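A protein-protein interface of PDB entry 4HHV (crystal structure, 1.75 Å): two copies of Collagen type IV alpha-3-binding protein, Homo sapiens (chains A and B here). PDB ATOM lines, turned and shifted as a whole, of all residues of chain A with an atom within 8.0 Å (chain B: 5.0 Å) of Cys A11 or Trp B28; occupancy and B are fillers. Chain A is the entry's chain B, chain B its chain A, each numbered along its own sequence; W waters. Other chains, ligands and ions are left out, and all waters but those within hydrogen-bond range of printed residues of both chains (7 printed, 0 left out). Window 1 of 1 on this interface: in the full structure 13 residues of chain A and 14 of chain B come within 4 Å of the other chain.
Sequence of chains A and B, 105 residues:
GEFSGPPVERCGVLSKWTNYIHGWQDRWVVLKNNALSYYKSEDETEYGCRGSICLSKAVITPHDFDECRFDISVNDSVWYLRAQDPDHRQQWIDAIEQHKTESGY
Glu A9 touches Val B30.
OE2 of Glu A9 touches OH of Tyr B39, at 3.8 Å.
O of Cys A11 touches CB of Tyr B47, 3.95 Å away.
Trp B28 touches Trp A28.
CZ3 of Trp A28 touches CE1 of Tyr B47, at 3.5 Å.
CE of Lys A32 touches SG of Cys B11 (3.7 Å).
Val B13 touches Glu A42 (CG2 to O, 3.4 Å).
Glu A42 touches Trp B28 (OE2 to CB, 3.6 Å).
Asp A43 touches Val B13 (OD1 to CG2, 3.9 Å).
Trp B28 touches Thr A45 (CH2 to CG2, 3.9 Å).
Of the 23 printed residues of chain A, 7 touch a printed residue of chain B.
Hydrophobic or aromatic side chains of chain A within 4 Å of the printed part of chain B: Trp A28.
Among the printed residues, 12 pairs touch across the chains.
Water W6 bridges the side-chain carboxylate of Glu A42 (2.4 Å) and the backbone carbonyl oxygen of Asp B26 (3.2 Å).
Water W3 bridges the side-chain carboxylate (OD1) of Asp A43 (2.5 Å) and the side-chain carboxylate (OD2) of Asp B26 (3.2 Å).
Water W2 lies within hydrogen-bond range of the side-chain hydroxyl of Tyr B39 (2.5 Å), the side-chain hydroxyl of Ser B37 (2.6 Å) and the side-chain carboxylate of Glu A9 (2.9 Å).
Water W7 lies within hydrogen-bond range of OH of Tyr B39 (2.7 Å) and OE1 of Glu A9 (2.8 Å).
Water W1 lies within hydrogen-bond range of the side-chain hydroxyl (OG1) of Thr A45 (2.7 Å) and the backbone carbonyl oxygen (O) of Cys B11 (2.8 Å).
Water W5 bridges OE2 of Glu A9 and OH of Tyr B39.
N of Tyr B39 sits at hydrogen-bond distance from O of Trp B28 (2.8 Å).
O of Val B30 is in hydrogen-bond range of N of Ser B37.
The backbone carbonyl oxygen (O) of Trp A28 sits at hydrogen-bond distance from the backbone NH (N) of Tyr A39 (2.9 Å).
OG of Ser A41 sits close to N of Asp A43, at 3.2 Å.
Cys A11 touches two residues of chain B.
Trp B28 touches just these residues of chain A: Cys A11 (3.6 Å), Trp A28 (3.5 Å), Glu A42 (3.6 Å) and Thr A45 (3.9 Å).
Of the printed residues of chain A, Tyr B39 touches Glu A9.
Of the printed residues of chain B, Lys A32 touches Cys B11.
Of the printed residues of chain A, Tyr B47 touches Cys A11, Trp A28 and Glu A42.
Of the printed residues of chain A, Cys B11 touches Lys A32 (3.7 Å).
The indole nitrogen (NE1) of Trp B28 sits close to the side-chain sulfur (SG) of Cys A11 (3.7 Å).
The side-chain hydroxyl of Tyr B47 sits at hydrogen-bond distance from the side-chain carboxylate of Glu A42 (3.1 Å).
Cys A11 touches Trp B28, but with the chains exchanged Trp A28 does not touch Cys B11 (6.9 Å).
Trp B28 touches its own counterpart, Trp A28.
9 positions are printed for both chains.
Of the 12 pairs that touch across the chains among the printed residues, 1 has its exchanged pair printed and touching as well.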
ATOM      1  N   GLU A   9      21.743 -30.883 -13.094  1.00  0.00           N
ATOM      2  CA  GLU A   9      21.556 -29.449 -13.339  1.00  0.00           C
ATOM      3  C   GLU A   9      20.936 -28.840 -12.092  1.00  0.00           C
ATOM      4  O   GLU A   9      20.241 -29.528 -11.337  1.00  0.00           O
ATOM      5  CB  GLU A   9      20.568 -29.190 -14.495  1.00  0.00           C
ATOM      6  CG  GLU A   9      20.912 -29.849 -15.821  1.00  0.00           C
ATOM      7  CD  GLU A   9      19.844 -29.540 -16.875  1.00  0.00           C
ATOM      8  OE1 GLU A   9      19.170 -30.482 -17.297  1.00  0.00           O
ATOM      9  OE2 GLU A   9      19.582 -28.363 -17.203  1.00  0.00           O
ATOM     10  N   ARG A  10      21.234 -27.581 -11.788  1.00  0.00           N
ATOM     11  CA  ARG A  10      20.498 -26.936 -10.709  1.00  0.00           C
ATOM     12  C   ARG A  10      20.679 -25.426 -10.822  1.00  0.00           C
ATOM     13  O   ARG A  10      21.770 -24.961 -11.175  1.00  0.00           O
ATOM     14  CB  ARG A  10      21.032 -27.404  -9.371  1.00  0.00           C
ATOM     15  CG  ARG A  10      20.148 -27.275  -8.118  1.00  0.00           C
ATOM     16  CD  ARG A  10      18.895 -28.016  -8.325  1.00  0.00           C
ATOM     17  NE  ARG A  10      19.114 -29.390  -8.839  1.00  0.00           N
ATOM     18  CZ  ARG A  10      18.680 -30.487  -8.278  1.00  0.00           C
ATOM     19  NH1 ARG A  10      17.976 -30.440  -7.129  1.00  0.00           N
ATOM     20  NH2 ARG A  10      18.876 -31.636  -8.910  1.00  0.00           N
ATOM     21  N   CYS A  11      19.621 -24.684 -10.540  1.00  0.00           N
ATOM     22  CA  CYS A  11      19.698 -23.244 -10.451  1.00  0.00           C
ATOM     23  C   CYS A  11      18.715 -22.816  -9.387  1.00  0.00           C
ATOM     24  O   CYS A  11      17.706 -23.475  -9.152  1.00  0.00           O
ATOM     25  CB  CYS A  11      19.414 -22.578 -11.763  1.00  0.00           C
ATOM     26  SG  CYS A  11      17.761 -22.849 -12.429  1.00  0.00           S
ATOM     27  N   GLY A  12      19.001 -21.684  -8.781  1.00  0.00           N
ATOM     28  CA  GLY A  12      18.074 -21.123  -7.802  1.00  0.00           C
ATOM     29  C   GLY A  12      18.735 -20.038  -6.988  1.00  0.00           C
ATOM     30  O   GLY A  12      19.930 -19.746  -7.160  1.00  0.00           O
ATOM     31  N   VAL A  13      17.965 -19.434  -6.088  1.00  0.00           N
ATOM     32  CA  VAL A  13      18.516 -18.443  -5.146  1.00  0.00           C
ATOM     33  C   VAL A  13      18.989 -19.111  -3.874  1.00  0.00           C
ATOM     34  O   VAL A  13      18.284 -19.964  -3.299  1.00  0.00           O
ATOM     35  CB  VAL A  13      17.519 -17.325  -4.835  1.00  0.00           C
ATOM     36  CG1 VAL A  13      18.067 -16.332  -3.797  1.00  0.00           C
ATOM     37  CG2 VAL A  13      17.096 -16.593  -6.106  1.00  0.00           C
ATOM     38  N   LEU A  14      20.196 -18.743  -3.453  1.00  0.00           N
ATOM     39  CA  LEU A  14      20.709 -19.113  -2.136  1.00  0.00           C
ATOM     40  C   LEU A  14      21.121 -17.811  -1.419  1.00  0.00           C
ATOM     41  O   LEU A  14      21.575 -16.861  -2.066  1.00  0.00           O
ATOM     42  CB  LEU A  14      21.894 -20.068  -2.251  1.00  0.00           C
ATOM     43  CG  LEU A  14      21.550 -21.475  -2.752  1.00  0.00           C
ATOM     44  CD1 LEU A  14      22.830 -22.217  -3.062  1.00  0.00           C
ATOM     45  CD2 LEU A  14      20.688 -22.210  -1.699  1.00  0.00           C
ATOM     46  N   ARG A  27      21.803 -14.527  -3.706  1.00  0.00           N
ATOM     47  CA  ARG A  27      22.505 -14.646  -4.955  1.00  0.00           C
ATOM     48  C   ARG A  27      21.886 -15.722  -5.816  1.00  0.00           C
ATOM     49  O   ARG A  27      21.308 -16.666  -5.318  1.00  0.00           O
ATOM     50  CB  ARG A  27      23.955 -14.995  -4.709  1.00  0.00           C
ATOM     51  CG  ARG A  27      24.680 -14.000  -3.840  1.00  0.00           C
ATOM     52  CD  ARG A  27      24.953 -12.734  -4.603  1.00  0.00           C
ATOM     53  NE  ARG A  27      25.704 -11.707  -3.863  1.00  0.00           N
ATOM     54  CZ  ARG A  27      25.196 -10.564  -3.424  1.00  0.00           C
ATOM     55  NH1 ARG A  27      23.906 -10.285  -3.564  1.00  0.00           N
ATOM     56  NH2 ARG A  27      25.969  -9.713  -2.795  1.00  0.00           N
ATOM     57  N   TRP A  28      22.016 -15.552  -7.118  1.00  0.00           N
ATOM     58  CA  TRP A  28      21.577 -16.579  -8.072  1.00  0.00           C
ATOM     59  C   TRP A  28      22.720 -17.541  -8.259  1.00  0.00           C
ATOM     60  O   TRP A  28      23.805 -17.111  -8.579  1.00  0.00           O
ATOM     61  CB  TRP A  28      21.275 -15.911  -9.382  1.00  0.00           C
ATOM     62  CG  TRP A  28      20.772 -16.843 -10.455  1.00  0.00           C
ATOM     63  CD1 TRP A  28      21.404 -17.177 -11.670  1.00  0.00           C
ATOM     64  CD2 TRP A  28      19.498 -17.514 -10.509  1.00  0.00           C
ATOM     65  NE1 TRP A  28      20.630 -18.037 -12.394  1.00  0.00           N
ATOM     66  CE2 TRP A  28      19.460 -18.245 -11.766  1.00  0.00           C
ATOM     67  CE3 TRP A  28      18.398 -17.582  -9.666  1.00  0.00           C
ATOM     68  CZ2 TRP A  28      18.375 -19.020 -12.109  1.00  0.00           C
ATOM     69  CZ3 TRP A  28      17.324 -18.344 -10.046  1.00  0.00           C
ATOM     70  CH2 TRP A  28      17.315 -19.049 -11.244  1.00  0.00           C
ATOM     71  N   VAL A  29      22.458 -18.844  -8.082  1.00  0.00           N
ATOM     72  CA  VAL A  29      23.500 -19.866  -8.133  1.00  0.00           C
ATOM     73  C   VAL A  29      23.161 -20.902  -9.202  1.00  0.00           C
ATOM     74  O   VAL A  29      21.985 -21.329  -9.338  1.00  0.00           O
ATOM     75  CB  VAL A  29      23.664 -20.520  -6.733  1.00  0.00           C
ATOM     76  CG1 VAL A  29      24.700 -21.668  -6.778  1.00  0.00           C
ATOM     77  CG2 VAL A  29      23.981 -19.436  -5.679  1.00  0.00           C
ATOM     78  N   VAL A  30      24.168 -21.250 -10.010  1.00  0.00           N
ATOM     79  CA  VAL A  30      23.999 -22.181 -11.109  1.00  0.00           C
ATOM     80  C   VAL A  30      25.072 -23.270 -11.017  1.00  0.00           C
ATOM     81  O   VAL A  30      26.275 -22.952 -10.900  1.00  0.00           O
ATOM     82  CB  VAL A  30      24.101 -21.478 -12.467  1.00  0.00           C
ATOM     83  CG1 VAL A  30      23.819 -22.490 -13.588  1.00  0.00           C
ATOM     84  CG2 VAL A  30      23.035 -20.349 -12.555  1.00  0.00           C
ATOM     85  N   LEU A  31      24.637 -24.521 -11.130  1.00  0.00           N
ATOM     86  CA  LEU A  31      25.496 -25.717 -11.136  1.00  0.00           C
ATOM     87  C   LEU A  31      25.619 -26.195 -12.575  1.00  0.00           C
ATOM     88  O   LEU A  31      24.606 -26.570 -13.215  1.00  0.00           O
ATOM     89  CB  LEU A  31      24.887 -26.799 -10.257  1.00  0.00           C
ATOM     90  CG  LEU A  31      25.634 -28.114 -10.095  1.00  0.00           C
ATOM     91  CD1 LEU A  31      26.969 -27.968  -9.434  1.00  0.00           C
ATOM     92  CD2 LEU A  31      24.766 -29.053  -9.283  1.00  0.00           C
ATOM     93  N   LYS A  32      26.815 -26.084 -13.133  1.00  0.00           N
ATOM     94  CA  LYS A  32      27.088 -26.511 -14.499  1.00  0.00           C
ATOM     95  C   LYS A  32      28.579 -26.470 -14.734  1.00  0.00           C
ATOM     96  O   LYS A  32      29.339 -25.788 -14.032  1.00  0.00           O
ATOM     97  CB  LYS A  32      26.405 -25.592 -15.537  1.00  0.00           C
ATOM     98  CG  LYS A  32      26.723 -24.140 -15.398  1.00  0.00           C
ATOM     99  CD  LYS A  32      26.000 -23.335 -16.482  1.00  0.00           C
ATOM    100  CE  LYS A  32      26.194 -21.836 -16.318  1.00  0.00           C
ATOM    101  NZ  LYS A  32      27.437 -21.166 -16.792  1.00  0.00           N
ATOM    102  N   LEU A  36      30.239 -24.491  -9.508  1.00  0.00           N
ATOM    103  CA  LEU A  36      29.137 -23.733  -8.957  1.00  0.00           C
ATOM    104  C   LEU A  36      29.469 -22.253  -9.161  1.00  0.00           C
ATOM    105  O   LEU A  36      30.524 -21.794  -8.761  1.00  0.00           O
ATOM    106  CB  LEU A  36      28.974 -24.067  -7.477  1.00  0.00           C
ATOM    107  CG  LEU A  36      27.655 -23.682  -6.816  1.00  0.00           C
ATOM    108  CD1 LEU A  36      26.550 -24.610  -7.351  1.00  0.00           C
ATOM    109  CD2 LEU A  36      27.738 -23.747  -5.281  1.00  0.00           C
ATOM    110  N   SER A  37      28.581 -21.546  -9.837  1.00  0.00           N
ATOM    111  CA  SER A  37      28.783 -20.178 -10.215  1.00  0.00           C
ATOM    112  C   SER A  37      27.702 -19.338  -9.589  1.00  0.00           C
ATOM    113  O   SER A  37      26.593 -19.816  -9.372  1.00  0.00           O
ATOM    114  CB  SER A  37      28.723 -20.042 -11.743  1.00  0.00           C
ATOM    115  OG  SER A  37      29.817 -20.713 -12.406  1.00  0.00           O
ATOM    116  N   TYR A  39      25.877 -15.194  -9.193  1.00  0.00           N
ATOM    117  CA  TYR A  39      25.579 -13.907  -9.823  1.00  0.00           C
ATOM    118  C   TYR A  39      24.742 -13.088  -8.866  1.00  0.00           C
ATOM    119  O   TYR A  39      24.147 -13.608  -7.912  1.00  0.00           O
ATOM    120  CB  TYR A  39      24.754 -14.137 -11.093  1.00  0.00           C
ATOM    121  CG  TYR A  39      25.356 -15.176 -12.009  1.00  0.00           C
ATOM    122  CD1 TYR A  39      25.154 -16.548 -11.788  1.00  0.00           C
ATOM    123  CD2 TYR A  39      26.133 -14.822 -13.082  1.00  0.00           C
ATOM    124  CE1 TYR A  39      25.723 -17.492 -12.597  1.00  0.00           C
ATOM    125  CE2 TYR A  39      26.671 -15.770 -13.924  1.00  0.00           C
ATOM    126  CZ  TYR A  39      26.491 -17.109 -13.677  1.00  0.00           C
ATOM    127  OH  TYR A  39      27.050 -18.044 -14.539  1.00  0.00           O
ATOM    128  N   SER A  41      21.873 -11.781  -9.400  1.00  0.00           N
ATOM    129  CA  SER A  41      20.499 -12.197  -9.611  1.00  0.00           C
ATOM    130  C   SER A  41      20.368 -12.969 -10.910  1.00  0.00           C
ATOM    131  O   SER A  41      21.256 -12.970 -11.780  1.00  0.00           O
ATOM    132  CB  SER A  41      19.563 -10.956  -9.692  1.00  0.00           C
ATOM    133  OG  SER A  41      19.604 -10.444 -11.006  1.00  0.00           O
ATOM    134  N   GLU A  42      19.194 -13.566 -11.068  1.00  0.00           N
ATOM    135  CA  GLU A  42      18.830 -14.367 -12.252  1.00  0.00           C
ATOM    136  C   GLU A  42      19.007 -13.590 -13.570  1.00  0.00           C
ATOM    137  O   GLU A  42      19.287 -14.146 -14.631  1.00  0.00           O
ATOM    138  CB  GLU A  42      17.363 -14.741 -12.106  1.00  0.00           C
ATOM    139  CG  GLU A  42      16.936 -15.803 -13.062  1.00  0.00           C
ATOM    140  CD  GLU A  42      15.439 -15.897 -13.228  1.00  0.00           C
ATOM    141  OE1 GLU A  42      14.740 -15.371 -12.336  1.00  0.00           O
ATOM    142  OE2 GLU A  42      14.952 -16.528 -14.194  1.00  0.00           O
ATOM    143  N   ASP A  43      18.835 -12.284 -13.489  1.00  0.00           N
ATOM    144  CA  ASP A  43      18.811 -11.466 -14.711  1.00  0.00           C
ATOM    145  C   ASP A  43      20.173 -10.935 -15.125  1.00  0.00           C
ATOM    146  O   ASP A  43      20.334 -10.297 -16.187  1.00  0.00           O
ATOM    147  CB  ASP A  43      17.904 -10.291 -14.492  1.00  0.00           C
ATOM    148  CG  ASP A  43      16.533 -10.716 -14.236  1.00  0.00           C
ATOM    149  OD1 ASP A  43      15.873 -11.157 -15.205  1.00  0.00           O
ATOM    150  OD2 ASP A  43      16.146 -10.655 -13.045  1.00  0.00           O
ATOM    151  N   GLU A  44      21.148 -11.218 -14.281  1.00  0.00           N
ATOM    152  CA  GLU A  44      22.466 -10.605 -14.407  1.00  0.00           C
ATOM    153  C   GLU A  44      23.529 -11.647 -14.674  1.00  0.00           C
ATOM    154  O   GLU A  44      24.635 -11.555 -14.156  1.00  0.00           O
ATOM    155  CB  GLU A  44      22.780  -9.798 -13.138  1.00  0.00           C
ATOM    156  CG  GLU A  44      21.965  -8.528 -13.004  1.00  0.00           C
ATOM    157  CD  GLU A  44      22.088  -7.892 -11.619  1.00  0.00           C
ATOM    158  OE1 GLU A  44      21.397  -8.315 -10.669  1.00  0.00           O
ATOM    159  OE2 GLU A  44      22.875  -6.931 -11.492  1.00  0.00           O
ATOM    160  N   THR A  45      23.219 -12.626 -15.510  1.00  0.00           N
ATOM    161  CA  THR A  45      24.200 -13.642 -15.794  1.00  0.00           C
ATOM    162  C   THR A  45      25.074 -13.313 -16.998  1.00  0.00           C
ATOM    163  O   THR A  45      26.102 -13.945 -17.175  1.00  0.00           O
ATOM    164  CB  THR A  45      23.540 -15.021 -15.959  1.00  0.00           C
ATOM    165  OG1 THR A  45      22.683 -15.056 -17.107  1.00  0.00           O
ATOM    166  CG2 THR A  45      22.744 -15.370 -14.677  1.00  0.00           C
ATOM    167  N   GLU A  46      24.687 -12.348 -17.810  1.00  0.00           N
ATOM    168  CA  GLU A  46      25.416 -12.167 -19.058  1.00  0.00           C
ATOM    169  C   GLU A  46      26.810 -11.644 -18.769  1.00  0.00           C
ATOM    170  O   GLU A  46      27.805 -12.223 -19.223  1.00  0.00           O
ATOM    171  CB  GLU A  46      24.680 -11.243 -20.014  1.00  0.00           C
ATOM    172  CG  GLU A  46      25.485 -11.010 -21.265  1.00  0.00           C
ATOM    173  CD  GLU A  46      24.687 -10.456 -22.403  1.00  0.00           C
ATOM    174  OE1 GLU A  46      23.521 -10.063 -22.192  1.00  0.00           O
ATOM    175  OE2 GLU A  46      25.260 -10.406 -23.499  1.00  0.00           O
ATOM    176  N   TRP A  92      20.371 -29.412  -2.780  1.00  0.00           N
ATOM    177  CA  TRP A  92      21.590 -28.796  -3.281  1.00  0.00           C
ATOM    178  C   TRP A  92      22.814 -29.616  -3.013  1.00  0.00           C
ATOM    179  O   TRP A  92      23.636 -29.793  -3.924  1.00  0.00           O
ATOM    180  CB  TRP A  92      21.763 -27.410  -2.702  1.00  0.00           C
ATOM    181  CG  TRP A  92      21.034 -26.312  -3.414  1.00  0.00           C
ATOM    182  CD1 TRP A  92      19.853 -25.671  -3.023  1.00  0.00           C
ATOM    183  CD2 TRP A  92      21.432 -25.669  -4.655  1.00  0.00           C
ATOM    184  NE1 TRP A  92      19.530 -24.682  -3.931  1.00  0.00           N
ATOM    185  CE2 TRP A  92      20.437 -24.653  -4.938  1.00  0.00           C
ATOM    186  CE3 TRP A  92      22.503 -25.808  -5.531  1.00  0.00           C
ATOM    187  CZ2 TRP A  92      20.521 -23.841  -6.060  1.00  0.00           C
ATOM    188  CZ3 TRP A  92      22.593 -24.950  -6.633  1.00  0.00           C
ATOM    189  CH2 TRP A  92      21.614 -24.005  -6.903  1.00  0.00           C
ATOM    190  N   ALA A  95      22.831 -32.655  -5.316  1.00  0.00           N
ATOM    191  CA  ALA A  95      23.071 -32.271  -6.712  1.00  0.00           C
ATOM    192  C   ALA A  95      24.555 -31.994  -6.939  1.00  0.00           C
ATOM    193  O   ALA A  95      25.160 -32.471  -7.902  1.00  0.00           O
ATOM    194  CB  ALA A  95      22.226 -31.058  -7.088  1.00  0.00           C
ATOM    195  N   CYS B  11      22.278 -20.996 -21.189  1.00  0.00           N
ATOM    196  CA  CYS B  11      21.212 -20.791 -20.242  1.00  0.00           C
ATOM    197  C   CYS B  11      21.065 -19.287 -20.075  1.00  0.00           C
ATOM    198  O   CYS B  11      22.045 -18.551 -20.138  1.00  0.00           O
ATOM    199  CB  CYS B  11      21.398 -21.477 -18.904  1.00  0.00           C
ATOM    200  SG  CYS B  11      22.962 -21.197 -18.091  1.00  0.00           S
ATOM    201  N   GLY B  12      19.850 -18.841 -19.841  1.00  0.00           N
ATOM    202  CA  GLY B  12      19.663 -17.395 -19.676  1.00  0.00           C
ATOM    203  C   GLY B  12      18.192 -17.076 -19.542  1.00  0.00           C
ATOM    204  O   GLY B  12      17.379 -17.949 -19.672  1.00  0.00           O
ATOM    205  N   VAL B  13      17.879 -15.810 -19.301  1.00  0.00           N
ATOM    206  CA  VAL B  13      16.504 -15.380 -19.272  1.00  0.00           C
ATOM    207  C   VAL B  13      15.993 -15.065 -20.673  1.00  0.00           C
ATOM    208  O   VAL B  13      16.679 -14.365 -21.453  1.00  0.00           O
ATOM    209  CB  VAL B  13      16.315 -14.166 -18.352  1.00  0.00           C
ATOM    210  CG1 VAL B  13      14.879 -13.582 -18.434  1.00  0.00           C
ATOM    211  CG2 VAL B  13      16.743 -14.504 -16.906  1.00  0.00           C
ATOM    212  N   ASP B  26       9.119 -13.492 -17.890  1.00  0.00           N
ATOM    213  CA  ASP B  26      10.491 -13.953 -17.961  1.00  0.00           C
ATOM    214  C   ASP B  26      10.632 -15.342 -17.391  1.00  0.00           C
ATOM    215  O   ASP B  26       9.998 -15.674 -16.369  1.00  0.00           O
ATOM    216  CB  ASP B  26      11.424 -13.054 -17.218  1.00  0.00           C
ATOM    217  CG  ASP B  26      11.833 -11.848 -18.038  1.00  0.00           C
ATOM    218  OD1 ASP B  26      11.651 -11.847 -19.263  1.00  0.00           O
ATOM    219  OD2 ASP B  26      12.379 -10.887 -17.442  1.00  0.00           O
ATOM    220  N   ARG B  27      11.395 -16.132 -18.101  1.00  0.00           N
ATOM    221  CA  ARG B  27      11.693 -17.483 -17.733  1.00  0.00           C
ATOM    222  C   ARG B  27      13.166 -17.779 -17.861  1.00  0.00           C
ATOM    223  O   ARG B  27      13.848 -17.227 -18.713  1.00  0.00           O
ATOM    224  CB  ARG B  27      10.892 -18.473 -18.634  1.00  0.00           C
ATOM    225  CG  ARG B  27       9.397 -18.279 -18.607  1.00  0.00           C
ATOM    226  CD  ARG B  27       8.784 -18.796 -17.340  1.00  0.00           C
ATOM    227  NE  ARG B  27       7.305 -18.596 -17.292  1.00  0.00           N
ATOM    228  CZ  ARG B  27       6.699 -17.750 -16.466  1.00  0.00           C
ATOM    229  NH1 ARG B  27       7.384 -16.944 -15.697  1.00  0.00           N
ATOM    230  NH2 ARG B  27       5.375 -17.711 -16.423  1.00  0.00           N
ATOM    231  N   TRP B  28      13.648 -18.739 -17.039  1.00  0.00           N
ATOM    232  CA  TRP B  28      15.000 -19.223 -17.178  1.00  0.00           C
ATOM    233  C   TRP B  28      14.960 -20.353 -18.189  1.00  0.00           C
ATOM    234  O   TRP B  28      14.264 -21.365 -17.967  1.00  0.00           O
ATOM    235  CB  TRP B  28      15.483 -19.721 -15.833  1.00  0.00           C
ATOM    236  CG  TRP B  28      16.906 -20.216 -15.796  1.00  0.00           C
ATOM    237  CD1 TRP B  28      17.346 -21.544 -15.746  1.00  0.00           C
ATOM    238  CD2 TRP B  28      18.102 -19.412 -15.882  1.00  0.00           C
ATOM    239  NE1 TRP B  28      18.740 -21.589 -15.745  1.00  0.00           N
ATOM    240  CE2 TRP B  28      19.232 -20.322 -15.797  1.00  0.00           C
ATOM    241  CE3 TRP B  28      18.357 -18.013 -15.888  1.00  0.00           C
ATOM    242  CZ2 TRP B  28      20.562 -19.844 -15.786  1.00  0.00           C
ATOM    243  CZ3 TRP B  28      19.684 -17.570 -15.893  1.00  0.00           C
ATOM    244  CH2 TRP B  28      20.744 -18.452 -15.836  1.00  0.00           C
ATOM    245  N   VAL B  29      15.701 -20.192 -19.268  1.00  0.00           N
ATOM    246  CA  VAL B  29      15.706 -21.116 -20.409  1.00  0.00           C
ATOM    247  C   VAL B  29      17.062 -21.765 -20.561  1.00  0.00           C
ATOM    248  O   VAL B  29      18.103 -21.147 -20.370  1.00  0.00           O
ATOM    249  CB  VAL B  29      15.259 -20.383 -21.708  1.00  0.00           C
ATOM    250  CG1 VAL B  29      15.243 -21.345 -22.928  1.00  0.00           C
ATOM    251  CG2 VAL B  29      13.846 -19.805 -21.505  1.00  0.00           C
ATOM    252  N   VAL B  30      17.063 -23.068 -20.843  1.00  0.00           N
ATOM    253  CA  VAL B  30      18.255 -23.871 -20.933  1.00  0.00           C
ATOM    254  C   VAL B  30      18.264 -24.692 -22.251  1.00  0.00           C
ATOM    255  O   VAL B  30      17.264 -25.317 -22.578  1.00  0.00           O
ATOM    256  CB  VAL B  30      18.367 -24.873 -19.771  1.00  0.00           C
ATOM    257  CG1 VAL B  30      19.595 -25.779 -19.956  1.00  0.00           C
ATOM    258  CG2 VAL B  30      18.413 -24.143 -18.405  1.00  0.00           C
ATOM    259  N   SER B  37      14.563 -26.285 -22.593  1.00  0.00           N
ATOM    260  CA  SER B  37      13.696 -26.386 -21.440  1.00  0.00           C
ATOM    261  C   SER B  37      13.566 -25.036 -20.744  1.00  0.00           C
ATOM    262  O   SER B  37      14.396 -24.139 -20.914  1.00  0.00           O
ATOM    263  CB  SER B  37      14.178 -27.479 -20.472  1.00  0.00           C
ATOM    264  OG  SER B  37      15.567 -27.339 -20.145  1.00  0.00           O
ATOM    265  N   TYR B  38      12.536 -24.899 -19.923  1.00  0.00           N
ATOM    266  CA  TYR B  38      12.391 -23.673 -19.132  1.00  0.00           C
ATOM    267  C   TYR B  38      11.929 -23.949 -17.691  1.00  0.00           C
ATOM    268  O   TYR B  38      11.294 -24.966 -17.398  1.00  0.00           O
ATOM    269  CB  TYR B  38      11.504 -22.645 -19.824  1.00  0.00           C
ATOM    270  CG  TYR B  38      10.041 -22.872 -19.749  1.00  0.00           C
ATOM    271  CD1 TYR B  38       9.260 -22.346 -18.725  1.00  0.00           C
ATOM    272  CD2 TYR B  38       9.417 -23.631 -20.682  1.00  0.00           C
ATOM    273  CE1 TYR B  38       7.902 -22.566 -18.685  1.00  0.00           C
ATOM    274  CE2 TYR B  38       8.048 -23.836 -20.664  1.00  0.00           C
ATOM    275  CZ  TYR B  38       7.300 -23.347 -19.659  1.00  0.00           C
ATOM    276  OH  TYR B  38       5.948 -23.573 -19.637  1.00  0.00           O
ATOM    277  N   TYR B  39      12.290 -23.018 -16.822  1.00  0.00           N
ATOM    278  CA  TYR B  39      12.163 -23.170 -15.391  1.00  0.00           C
ATOM    279  C   TYR B  39      11.350 -22.029 -14.837  1.00  0.00           C
ATOM    280  O   TYR B  39      11.454 -20.884 -15.322  1.00  0.00           O
ATOM    281  CB  TYR B  39      13.592 -23.204 -14.768  1.00  0.00           C
ATOM    282  CG  TYR B  39      14.310 -24.451 -15.114  1.00  0.00           C
ATOM    283  CD1 TYR B  39      14.833 -24.667 -16.379  1.00  0.00           C
ATOM    284  CD2 TYR B  39      14.412 -25.486 -14.148  1.00  0.00           C
ATOM    285  CE1 TYR B  39      15.412 -25.908 -16.698  1.00  0.00           C
ATOM    286  CE2 TYR B  39      14.982 -26.690 -14.465  1.00  0.00           C
ATOM    287  CZ  TYR B  39      15.489 -26.876 -15.717  1.00  0.00           C
ATOM    288  OH  TYR B  39      16.033 -28.132 -15.930  1.00  0.00           O
ATOM    289  N   TYR B  47      13.330 -23.346  -8.039  1.00  0.00           N
ATOM    290  CA  TYR B  47      12.901 -23.458  -9.423  1.00  0.00           C
ATOM    291  C   TYR B  47      12.668 -24.892  -9.793  1.00  0.00           C
ATOM    292  O   TYR B  47      13.188 -25.797  -9.159  1.00  0.00           O
ATOM    293  CB  TYR B  47      13.979 -22.841 -10.299  1.00  0.00           C
ATOM    294  CG  TYR B  47      13.953 -21.326 -10.238  1.00  0.00           C
ATOM    295  CD1 TYR B  47      14.264 -20.635  -9.074  1.00  0.00           C
ATOM    296  CD2 TYR B  47      13.471 -20.592 -11.316  1.00  0.00           C
ATOM    297  CE1 TYR B  47      14.127 -19.249  -9.019  1.00  0.00           C
ATOM    298  CE2 TYR B  47      13.384 -19.221 -11.292  1.00  0.00           C
ATOM    299  CZ  TYR B  47      13.691 -18.547 -10.122  1.00  0.00           C
ATOM    300  OH  TYR B  47      13.598 -17.151 -10.038  1.00  0.00           O
HETATM  301  O   HOH W   1      23.223 -16.036 -19.601  1.00  0.00           O
HETATM  302  O   HOH W   2      16.912 -28.579 -18.232  1.00  0.00           O
HETATM  303  O   HOH W   3      13.636 -12.133 -14.734  1.00  0.00           O
HETATM  304  O   HOH W   4      11.719 -15.897 -11.460  1.00  0.00           O
HETATM  305  O   HOH W   5      18.738 -26.342 -15.373  1.00  0.00           O
HETATM  306  O   HOH W   6      12.552 -16.379 -14.598  1.00  0.00           O
HETATM  307  O   HOH W   7      17.216 -30.466 -15.295  1.00  0.00           O
